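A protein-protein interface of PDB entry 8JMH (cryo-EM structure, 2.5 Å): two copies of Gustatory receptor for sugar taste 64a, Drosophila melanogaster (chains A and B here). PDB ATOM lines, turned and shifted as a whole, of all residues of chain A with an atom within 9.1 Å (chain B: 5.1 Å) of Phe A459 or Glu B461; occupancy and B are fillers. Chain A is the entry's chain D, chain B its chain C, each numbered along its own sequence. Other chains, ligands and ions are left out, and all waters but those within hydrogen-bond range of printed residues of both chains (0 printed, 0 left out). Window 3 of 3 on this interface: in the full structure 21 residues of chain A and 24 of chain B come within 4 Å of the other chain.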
ATOM      1  N   ALA A 143      -2.026  20.254   6.167  1.00  0.00           N
ATOM      2  CA  ALA A 143      -3.003  21.319   5.975  1.00  0.00           C
ATOM      3  C   ALA A 143      -3.579  21.321   4.567  1.00  0.00           C
ATOM      4  O   ALA A 143      -4.686  21.829   4.363  1.00  0.00           O
ATOM      5  CB  ALA A 143      -2.366  22.676   6.277  1.00  0.00           C
ATOM      6  N   LYS A 144      -2.857  20.766   3.594  1.00  0.00           N
ATOM      7  CA  LYS A 144      -3.354  20.682   2.227  1.00  0.00           C
ATOM      8  C   LYS A 144      -4.232  19.460   2.002  1.00  0.00           C
ATOM      9  O   LYS A 144      -5.218  19.544   1.260  1.00  0.00           O
ATOM     10  CB  LYS A 144      -2.179  20.652   1.244  1.00  0.00           C
ATOM     11  CG  LYS A 144      -2.062  21.899   0.386  1.00  0.00           C
ATOM     12  CD  LYS A 144      -1.381  23.026   1.146  1.00  0.00           C
ATOM     13  CE  LYS A 144      -1.903  24.384   0.711  1.00  0.00           C
ATOM     14  NZ  LYS A 144      -1.207  25.500   1.408  1.00  0.00           N
ATOM     15  N   LEU A 356      -5.283  31.043   0.194  1.00  0.00           N
ATOM     16  CA  LEU A 356      -3.917  30.708   0.569  1.00  0.00           C
ATOM     17  C   LEU A 356      -3.120  30.093  -0.574  1.00  0.00           C
ATOM     18  O   LEU A 356      -1.894  29.990  -0.461  1.00  0.00           O
ATOM     19  CB  LEU A 356      -3.922  29.747   1.759  1.00  0.00           C
ATOM     20  CG  LEU A 356      -2.923  30.027   2.884  1.00  0.00           C
ATOM     21  CD1 LEU A 356      -3.128  31.405   3.502  1.00  0.00           C
ATOM     22  CD2 LEU A 356      -3.021  28.944   3.947  1.00  0.00           C
ATOM     23  N   TYR A 452      -6.855  36.876   8.339  1.00  0.00           N
ATOM     24  CA  TYR A 452      -6.457  35.476   8.402  1.00  0.00           C
ATOM     25  C   TYR A 452      -5.482  35.136   7.286  1.00  0.00           C
ATOM     26  O   TYR A 452      -4.512  34.409   7.507  1.00  0.00           O
ATOM     27  CB  TYR A 452      -7.686  34.568   8.325  1.00  0.00           C
ATOM     28  CG  TYR A 452      -8.582  34.597   9.546  1.00  0.00           C
ATOM     29  CD1 TYR A 452      -8.235  35.318  10.681  1.00  0.00           C
ATOM     30  CD2 TYR A 452      -9.778  33.892   9.562  1.00  0.00           C
ATOM     31  CE1 TYR A 452      -9.053  35.338  11.791  1.00  0.00           C
ATOM     32  CE2 TYR A 452     -10.602  33.908  10.667  1.00  0.00           C
ATOM     33  CZ  TYR A 452     -10.235  34.632  11.779  1.00  0.00           C
ATOM     34  OH  TYR A 452     -11.054  34.651  12.883  1.00  0.00           O
ATOM     35  N   GLU A 453      -5.727  35.642   6.077  1.00  0.00           N
ATOM     36  CA  GLU A 453      -4.824  35.364   4.967  1.00  0.00           C
ATOM     37  C   GLU A 453      -3.461  36.001   5.192  1.00  0.00           C
ATOM     38  O   GLU A 453      -2.430  35.382   4.915  1.00  0.00           O
ATOM     39  CB  GLU A 453      -5.438  35.856   3.657  1.00  0.00           C
ATOM     40  CG  GLU A 453      -6.601  35.011   3.174  1.00  0.00           C
ATOM     41  CD  GLU A 453      -6.214  33.563   2.959  1.00  0.00           C
ATOM     42  OE1 GLU A 453      -5.197  33.315   2.279  1.00  0.00           O
ATOM     43  OE2 GLU A 453      -6.914  32.676   3.484  1.00  0.00           O
ATOM     44  N   LEU A 454      -3.433  37.236   5.698  1.00  0.00           N
ATOM     45  CA  LEU A 454      -2.154  37.877   5.978  1.00  0.00           C
ATOM     46  C   LEU A 454      -1.361  37.080   7.003  1.00  0.00           C
ATOM     47  O   LEU A 454      -0.146  36.902   6.857  1.00  0.00           O
ATOM     48  CB  LEU A 454      -2.377  39.307   6.471  1.00  0.00           C
ATOM     49  CG  LEU A 454      -2.840  40.335   5.438  1.00  0.00           C
ATOM     50  CD1 LEU A 454      -3.059  41.683   6.101  1.00  0.00           C
ATOM     51  CD2 LEU A 454      -1.837  40.456   4.303  1.00  0.00           C
ATOM     52  N   VAL A 455      -2.028  36.593   8.048  1.00  0.00           N
ATOM     53  CA  VAL A 455      -1.319  35.812   9.057  1.00  0.00           C
ATOM     54  C   VAL A 455      -0.898  34.447   8.514  1.00  0.00           C
ATOM     55  O   VAL A 455       0.196  33.965   8.826  1.00  0.00           O
ATOM     56  CB  VAL A 455      -2.181  35.664  10.321  1.00  0.00           C
ATOM     57  CG1 VAL A 455      -1.491  34.760  11.328  1.00  0.00           C
ATOM     58  CG2 VAL A 455      -2.459  37.026  10.933  1.00  0.00           C
ATOM     59  N   LEU A 456      -1.741  33.805   7.702  1.00  0.00           N
ATOM     60  CA  LEU A 456      -1.491  32.433   7.278  1.00  0.00           C
ATOM     61  C   LEU A 456      -0.496  32.344   6.131  1.00  0.00           C
ATOM     62  O   LEU A 456       0.152  31.304   5.966  1.00  0.00           O
ATOM     63  CB  LEU A 456      -2.805  31.771   6.863  1.00  0.00           C
ATOM     64  CG  LEU A 456      -3.723  31.288   7.983  1.00  0.00           C
ATOM     65  CD1 LEU A 456      -5.105  30.981   7.435  1.00  0.00           C
ATOM     66  CD2 LEU A 456      -3.135  30.063   8.660  1.00  0.00           C
ATOM     67  N   LEU A 457      -0.362  33.394   5.321  1.00  0.00           N
ATOM     68  CA  LEU A 457       0.572  33.325   4.203  1.00  0.00           C
ATOM     69  C   LEU A 457       1.996  33.101   4.688  1.00  0.00           C
ATOM     70  O   LEU A 457       2.823  32.555   3.950  1.00  0.00           O
ATOM     71  CB  LEU A 457       0.478  34.595   3.361  1.00  0.00           C
ATOM     72  CG  LEU A 457      -0.691  34.642   2.374  1.00  0.00           C
ATOM     73  CD1 LEU A 457      -0.873  36.049   1.834  1.00  0.00           C
ATOM     74  CD2 LEU A 457      -0.484  33.655   1.236  1.00  0.00           C
ATOM     75  N   GLN A 458       2.301  33.504   5.923  1.00  0.00           N
ATOM     76  CA  GLN A 458       3.597  33.180   6.510  1.00  0.00           C
ATOM     77  C   GLN A 458       3.748  31.675   6.699  1.00  0.00           C
ATOM     78  O   GLN A 458       4.833  31.119   6.491  1.00  0.00           O
ATOM     79  CB  GLN A 458       3.766  33.913   7.840  1.00  0.00           C
ATOM     80  CG  GLN A 458       3.975  35.410   7.694  1.00  0.00           C
ATOM     81  CD  GLN A 458       3.399  36.199   8.852  1.00  0.00           C
ATOM     82  OE1 GLN A 458       3.170  35.661   9.934  1.00  0.00           O
ATOM     83  NE2 GLN A 458       3.166  37.487   8.629  1.00  0.00           N
ATOM     84  N   PHE A 459       2.668  30.998   7.097  1.00  0.00           N
ATOM     85  CA  PHE A 459       2.719  29.548   7.249  1.00  0.00           C
ATOM     86  C   PHE A 459       3.047  28.866   5.928  1.00  0.00           C
ATOM     87  O   PHE A 459       3.820  27.902   5.890  1.00  0.00           O
ATOM     88  CB  PHE A 459       1.384  29.023   7.784  1.00  0.00           C
ATOM     89  CG  PHE A 459       1.224  29.161   9.267  1.00  0.00           C
ATOM     90  CD1 PHE A 459       1.730  28.200  10.124  1.00  0.00           C
ATOM     91  CD2 PHE A 459       0.553  30.245   9.807  1.00  0.00           C
ATOM     92  CE1 PHE A 459       1.578  28.322  11.489  1.00  0.00           C
ATOM     93  CE2 PHE A 459       0.397  30.371  11.171  1.00  0.00           C
ATOM     94  CZ  PHE A 459       0.910  29.407  12.013  1.00  0.00           C
ATOM     95  N   ASP A 460       2.464  29.349   4.834  1.00  0.00           N
ATOM     96  CA  ASP A 460       2.568  28.701   3.535  1.00  0.00           C
ATOM     97  C   ASP A 460       3.767  29.172   2.721  1.00  0.00           C
ATOM     98  O   ASP A 460       3.930  28.731   1.578  1.00  0.00           O
ATOM     99  CB  ASP A 460       1.280  28.934   2.737  1.00  0.00           C
ATOM    100  CG  ASP A 460       1.063  27.892   1.659  1.00  0.00           C
ATOM    101  OD1 ASP A 460       0.800  26.721   2.007  1.00  0.00           O
ATOM    102  OD2 ASP A 460       1.146  28.242   0.464  1.00  0.00           O
ATOM    103  N   GLU A 461       4.607  30.056   3.273  1.00  0.00           N
ATOM    104  CA  GLU A 461       5.773  30.518   2.518  1.00  0.00           C
ATOM    105  C   GLU A 461       6.691  29.369   2.127  1.00  0.00           C
ATOM    106  O   GLU A 461       7.124  29.320   0.961  1.00  0.00           O
ATOM    107  CB  GLU A 461       6.524  31.583   3.320  1.00  0.00           C
ATOM    108  CG  GLU A 461       5.949  32.984   3.188  1.00  0.00           C
ATOM    109  CD  GLU A 461       6.833  34.040   3.822  1.00  0.00           C
ATOM    110  OE1 GLU A 461       8.057  33.812   3.924  1.00  0.00           O
ATOM    111  OE2 GLU A 461       6.304  35.099   4.220  1.00  0.00           O
ATOM    112  N   PRO A 462       7.047  28.438   3.018  1.00  0.00           N
ATOM    113  CA  PRO A 462       7.930  27.335   2.600  1.00  0.00           C
ATOM    114  C   PRO A 462       7.395  26.552   1.412  1.00  0.00           C
ATOM    115  O   PRO A 462       8.073  26.449   0.382  1.00  0.00           O
ATOM    116  CB  PRO A 462       8.026  26.472   3.867  1.00  0.00           C
ATOM    117  CG  PRO A 462       7.749  27.405   4.988  1.00  0.00           C
ATOM    118  CD  PRO A 462       6.766  28.406   4.464  1.00  0.00           C
ATOM    119  N   ASN A 463       6.183  26.003   1.527  1.00  0.00           N
ATOM    120  CA  ASN A 463       5.602  25.254   0.421  1.00  0.00           C
ATOM    121  C   ASN A 463       5.435  26.112  -0.824  1.00  0.00           C
ATOM    122  O   ASN A 463       5.520  25.587  -1.939  1.00  0.00           O
ATOM    123  CB  ASN A 463       4.250  24.668   0.833  1.00  0.00           C
ATOM    124  CG  ASN A 463       4.373  23.648   1.951  1.00  0.00           C
ATOM    125  OD1 ASN A 463       4.321  22.442   1.713  1.00  0.00           O
ATOM    126  ND2 ASN A 463       4.530  24.130   3.179  1.00  0.00           N
ATOM    127  N   ARG A 464       5.201  27.416  -0.661  1.00  0.00           N
ATOM    128  CA  ARG A 464       5.132  28.300  -1.819  1.00  0.00           C
ATOM    129  C   ARG A 464       6.469  28.363  -2.544  1.00  0.00           C
ATOM    130  O   ARG A 464       6.515  28.298  -3.778  1.00  0.00           O
ATOM    131  CB  ARG A 464       4.697  29.700  -1.388  1.00  0.00           C
ATOM    132  CG  ARG A 464       3.200  29.931  -1.442  1.00  0.00           C
ATOM    133  CD  ARG A 464       2.826  31.246  -0.781  1.00  0.00           C
ATOM    134  NE  ARG A 464       3.538  32.372  -1.375  1.00  0.00           N
ATOM    135  CZ  ARG A 464       3.807  33.510  -0.748  1.00  0.00           C
ATOM    136  NH1 ARG A 464       3.432  33.718   0.503  1.00  0.00           N
ATOM    137  NH2 ARG A 464       4.469  34.465  -1.396  1.00  0.00           N
ATOM    138  N   ARG A 465       7.568  28.490  -1.797  1.00  0.00           N
ATOM    139  CA  ARG A 465       8.879  28.591  -2.425  1.00  0.00           C
ATOM    140  C   ARG A 465       9.399  27.248  -2.919  1.00  0.00           C
ATOM    141  O   ARG A 465      10.298  27.224  -3.768  1.00  0.00           O
ATOM    142  CB  ARG A 465       9.893  29.209  -1.457  1.00  0.00           C
ATOM    143  CG  ARG A 465      10.099  28.434  -0.167  1.00  0.00           C
ATOM    144  CD  ARG A 465      11.342  28.913   0.568  1.00  0.00           C
ATOM    145  NE  ARG A 465      11.747  27.988   1.622  1.00  0.00           N
ATOM    146  CZ  ARG A 465      11.454  28.130   2.909  1.00  0.00           C
ATOM    147  NH1 ARG A 465      10.741  29.154   3.351  1.00  0.00           N
ATOM    148  NH2 ARG A 465      11.888  27.220   3.776  1.00  0.00           N
ATOM    149  N   LYS A 466       8.864  26.133  -2.414  1.00  0.00           N
ATOM    150  CA  LYS A 466       9.270  24.834  -2.944  1.00  0.00           C
ATOM    151  C   LYS A 466       8.937  24.712  -4.425  1.00  0.00           C
ATOM    152  O   LYS A 466       9.679  24.072  -5.178  1.00  0.00           O
ATOM    153  CB  LYS A 466       8.602  23.698  -2.164  1.00  0.00           C
ATOM    154  CG  LYS A 466       8.928  23.643  -0.674  1.00  0.00           C
ATOM    155  CD  LYS A 466      10.383  23.979  -0.378  1.00  0.00           C
ATOM    156  CE  LYS A 466      10.723  23.726   1.083  1.00  0.00           C
ATOM    157  NZ  LYS A 466      11.244  24.949   1.755  1.00  0.00           N
ATOM    158  N   LEU B 454      -3.731  31.618  15.316  1.00  0.00           N
ATOM    159  CA  LEU B 454      -3.016  31.764  14.053  1.00  0.00           C
ATOM    160  C   LEU B 454      -1.680  32.463  14.264  1.00  0.00           C
ATOM    161  O   LEU B 454      -0.655  32.038  13.717  1.00  0.00           O
ATOM    162  CB  LEU B 454      -3.872  32.540  13.052  1.00  0.00           C
ATOM    163  CG  LEU B 454      -5.106  31.822  12.505  1.00  0.00           C
ATOM    164  CD1 LEU B 454      -5.886  32.745  11.583  1.00  0.00           C
ATOM    165  CD2 LEU B 454      -4.716  30.548  11.781  1.00  0.00           C
ATOM    166  N   LEU B 457       0.595  30.146  16.698  1.00  0.00           N
ATOM    167  CA  LEU B 457       1.103  28.897  16.141  1.00  0.00           C
ATOM    168  C   LEU B 457       2.472  29.088  15.505  1.00  0.00           C
ATOM    169  O   LEU B 457       3.262  28.140  15.439  1.00  0.00           O
ATOM    170  CB  LEU B 457       0.110  28.330  15.126  1.00  0.00           C
ATOM    171  CG  LEU B 457      -1.045  27.518  15.716  1.00  0.00           C
ATOM    172  CD1 LEU B 457      -2.105  27.262  14.660  1.00  0.00           C
ATOM    173  CD2 LEU B 457      -0.545  26.206  16.301  1.00  0.00           C
ATOM    174  N   GLN B 458       2.774  30.300  15.035  1.00  0.00           N
ATOM    175  CA  GLN B 458       4.114  30.586  14.534  1.00  0.00           C
ATOM    176  C   GLN B 458       5.146  30.486  15.651  1.00  0.00           C
ATOM    177  O   GLN B 458       6.264  30.005  15.436  1.00  0.00           O
ATOM    178  CB  GLN B 458       4.146  31.971  13.888  1.00  0.00           C
ATOM    179  CG  GLN B 458       3.433  32.041  12.550  1.00  0.00           C
ATOM    180  CD  GLN B 458       2.799  33.394  12.293  1.00  0.00           C
ATOM    181  OE1 GLN B 458       3.176  34.396  12.901  1.00  0.00           O
ATOM    182  NE2 GLN B 458       1.831  33.430  11.385  1.00  0.00           N
ATOM    183  N   PHE B 459       4.787  30.938  16.855  1.00  0.00           N
ATOM    184  CA  PHE B 459       5.698  30.831  17.989  1.00  0.00           C
ATOM    185  C   PHE B 459       6.034  29.378  18.293  1.00  0.00           C
ATOM    186  O   PHE B 459       7.183  29.048  18.606  1.00  0.00           O
ATOM    187  CB  PHE B 459       5.082  31.489  19.225  1.00  0.00           C
ATOM    188  CG  PHE B 459       5.229  32.980  19.260  1.00  0.00           C
ATOM    189  CD1 PHE B 459       6.381  33.563  19.757  1.00  0.00           C
ATOM    190  CD2 PHE B 459       4.209  33.798  18.809  1.00  0.00           C
ATOM    191  CE1 PHE B 459       6.516  34.935  19.796  1.00  0.00           C
ATOM    192  CE2 PHE B 459       4.339  35.171  18.846  1.00  0.00           C
ATOM    193  CZ  PHE B 459       5.494  35.739  19.340  1.00  0.00           C
ATOM    194  N   ASP B 460       5.041  28.496  18.213  1.00  0.00           N
ATOM    195  CA  ASP B 460       5.193  27.105  18.615  1.00  0.00           C
ATOM    196  C   ASP B 460       5.698  26.207  17.492  1.00  0.00           C
ATOM    197  O   ASP B 460       5.850  25.001  17.709  1.00  0.00           O
ATOM    198  CB  ASP B 460       3.856  26.569  19.139  1.00  0.00           C
ATOM    199  CG  ASP B 460       4.022  25.360  20.038  1.00  0.00           C
ATOM    200  OD1 ASP B 460       4.546  25.521  21.160  1.00  0.00           O
ATOM    201  OD2 ASP B 460       3.622  24.252  19.627  1.00  0.00           O
ATOM    202  N   GLU B 461       5.957  26.756  16.300  1.00  0.00           N
ATOM    203  CA  GLU B 461       6.451  25.918  15.207  1.00  0.00           C
ATOM    204  C   GLU B 461       7.761  25.230  15.564  1.00  0.00           C
ATOM    205  O   GLU B 461       7.877  24.014  15.333  1.00  0.00           O
ATOM    206  CB  GLU B 461       6.589  26.754  13.931  1.00  0.00           C
ATOM    207  CG  GLU B 461       5.297  26.917  13.149  1.00  0.00           C
ATOM    208  CD  GLU B 461       5.514  27.577  11.802  1.00  0.00           C
ATOM    209  OE1 GLU B 461       6.638  27.483  11.264  1.00  0.00           O
ATOM    210  OE2 GLU B 461       4.561  28.192  11.279  1.00  0.00           O
ATOM    211  N   PRO B 462       8.772  25.916  16.106  1.00  0.00           N
ATOM    212  CA  PRO B 462      10.024  25.213  16.444  1.00  0.00           C
ATOM    213  C   PRO B 462       9.815  23.995  17.329  1.00  0.00           C
ATOM    214  O   PRO B 462      10.239  22.891  16.969  1.00  0.00           O
ATOM    215  CB  PRO B 462      10.849  26.303  17.140  1.00  0.00           C
ATOM    216  CG  PRO B 462      10.337  27.580  16.587  1.00  0.00           C
ATOM    217  CD  PRO B 462       8.875  27.369  16.326  1.00  0.00           C
ATOM    218  N   ASN B 463       9.162  24.166  18.480  1.00  0.00           N
ATOM    219  CA  ASN B 463       8.921  23.035  19.368  1.00  0.00           C
ATOM    220  C   ASN B 463       8.048  21.970  18.718  1.00  0.00           C
ATOM    221  O   ASN B 463       8.191  20.788  19.042  1.00  0.00           O
ATOM    222  CB  ASN B 463       8.271  23.515  20.668  1.00  0.00           C
ATOM    223  CG  ASN B 463       9.185  24.417  21.477  1.00  0.00           C
ATOM    224  OD1 ASN B 463       9.783  23.988  22.464  1.00  0.00           O
ATOM    225  ND2 ASN B 463       9.294  25.675  21.066  1.00  0.00           N
ATOM    226  N   ARG B 464       7.151  22.362  17.810  1.00  0.00           N
ATOM    227  CA  ARG B 464       6.312  21.380  17.130  1.00  0.00           C
ATOM    228  C   ARG B 464       7.146  20.439  16.270  1.00  0.00           C
ATOM    229  O   ARG B 464       6.910  19.225  16.263  1.00  0.00           O
ATOM    230  CB  ARG B 464       5.262  22.090  16.277  1.00  0.00           C
ATOM    231  CG  ARG B 464       3.940  22.322  16.985  1.00  0.00           C
ATOM    232  CD  ARG B 464       3.038  23.237  16.176  1.00  0.00           C
ATOM    233  NE  ARG B 464       2.808  22.725  14.828  1.00  0.00           N
ATOM    234  CZ  ARG B 464       2.503  23.476  13.779  1.00  0.00           C
ATOM    235  NH1 ARG B 464       2.372  24.789  13.881  1.00  0.00           N
ATOM    236  NH2 ARG B 464       2.323  22.895  12.596  1.00  0.00           N
ATOM    237  N   ARG B 465       8.122  20.977  15.537  1.00  0.00           N
ATOM    238  CA  ARG B 465       8.925  20.152  14.643  1.00  0.00           C
ATOM    239  C   ARG B 465       9.972  19.328  15.380  1.00  0.00           C
ATOM    240  O   ARG B 465      10.500  18.371  14.805  1.00  0.00           O
ATOM    241  CB  ARG B 465       9.608  21.027  13.587  1.00  0.00           C
ATOM    242  CG  ARG B 465      10.494  22.127  14.148  1.00  0.00           C
ATOM    243  CD  ARG B 465      11.383  22.719  13.067  1.00  0.00           C
ATOM    244  NE  ARG B 465      12.458  23.535  13.623  1.00  0.00           N
ATOM    245  CZ  ARG B 465      12.434  24.859  13.716  1.00  0.00           C
ATOM    246  NH1 ARG B 465      11.396  25.568  13.301  1.00  0.00           N
ATOM    247  NH2 ARG B 465      13.480  25.490  14.241  1.00  0.00           N
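NE2 of Gln B458 lies within hydrogen-bond range of O of Val A455.
NE2 of Gln B458 is in hydrogen-bond range of OE1 of Gln A458, 3.0 Å away.
Among the printed residues, pairs that only touch across the chains: Phe A459 with Glu B461 (3.0 Å), Phe A459 with Leu B454 (3.2 Å), Phe A459 with Gln B458 (3.4 Å), Phe A459 with Leu B457 (3.4 Å), Leu A456 with Leu B454 (3.5 Å), Tyr A452 with Leu B454 (3.6 Å) and Val A455 with Leu B454 (3.7 Å).
Of chain B, only Leu B454, Leu B457, Gln B458 and Glu B461 come within 4 Å of Phe A459.
Of chain A, only Phe A459 comes within 4 Å of Glu B461.
No residue of chain A comes within 4 Å of Pro B462.
No residue of chain A comes within 4 Å of Arg B464.
Of the printed residues of chain A, Leu B454 touches Tyr A452, Val A455, Leu A456 and Phe A459.
Printed residues of chain A within 4 Å of Leu B457: Phe A459.
Of the printed residues of chain B, Gln A458 touches Gln B458 (3.0 Å).
Asp B460 touches none of the printed residues of chain A.
The nearest residue of chain B that does not touch Phe A459 is Arg B464 (4.3 Å).
The nearest printed residue of chain B that does not touch Gln A458 is Glu B461 (5.6 Å).
Of the 18 printed residues of chain A, 5 touch a printed residue of chain B.
Hydrophobic or aromatic side chains of chain A within 4 Å of the printed part of chain B: Tyr A452, Val A455, Leu A456 and Phe A459.
Gln A458 touches its own counterpart, Gln B458.
Phe A459 touches Leu B454, but with the chains exchanged Leu A454 does not touch Phe B459 (12.6 Å).
Phe A459 touches Leu B457, but with the chains exchanged Leu A457 does not touch Phe B459 (12.7 Å).
Phe A459 touches Glu B461, but with the chains exchanged Glu A461 does not touch Phe B459 (13.4 Å).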
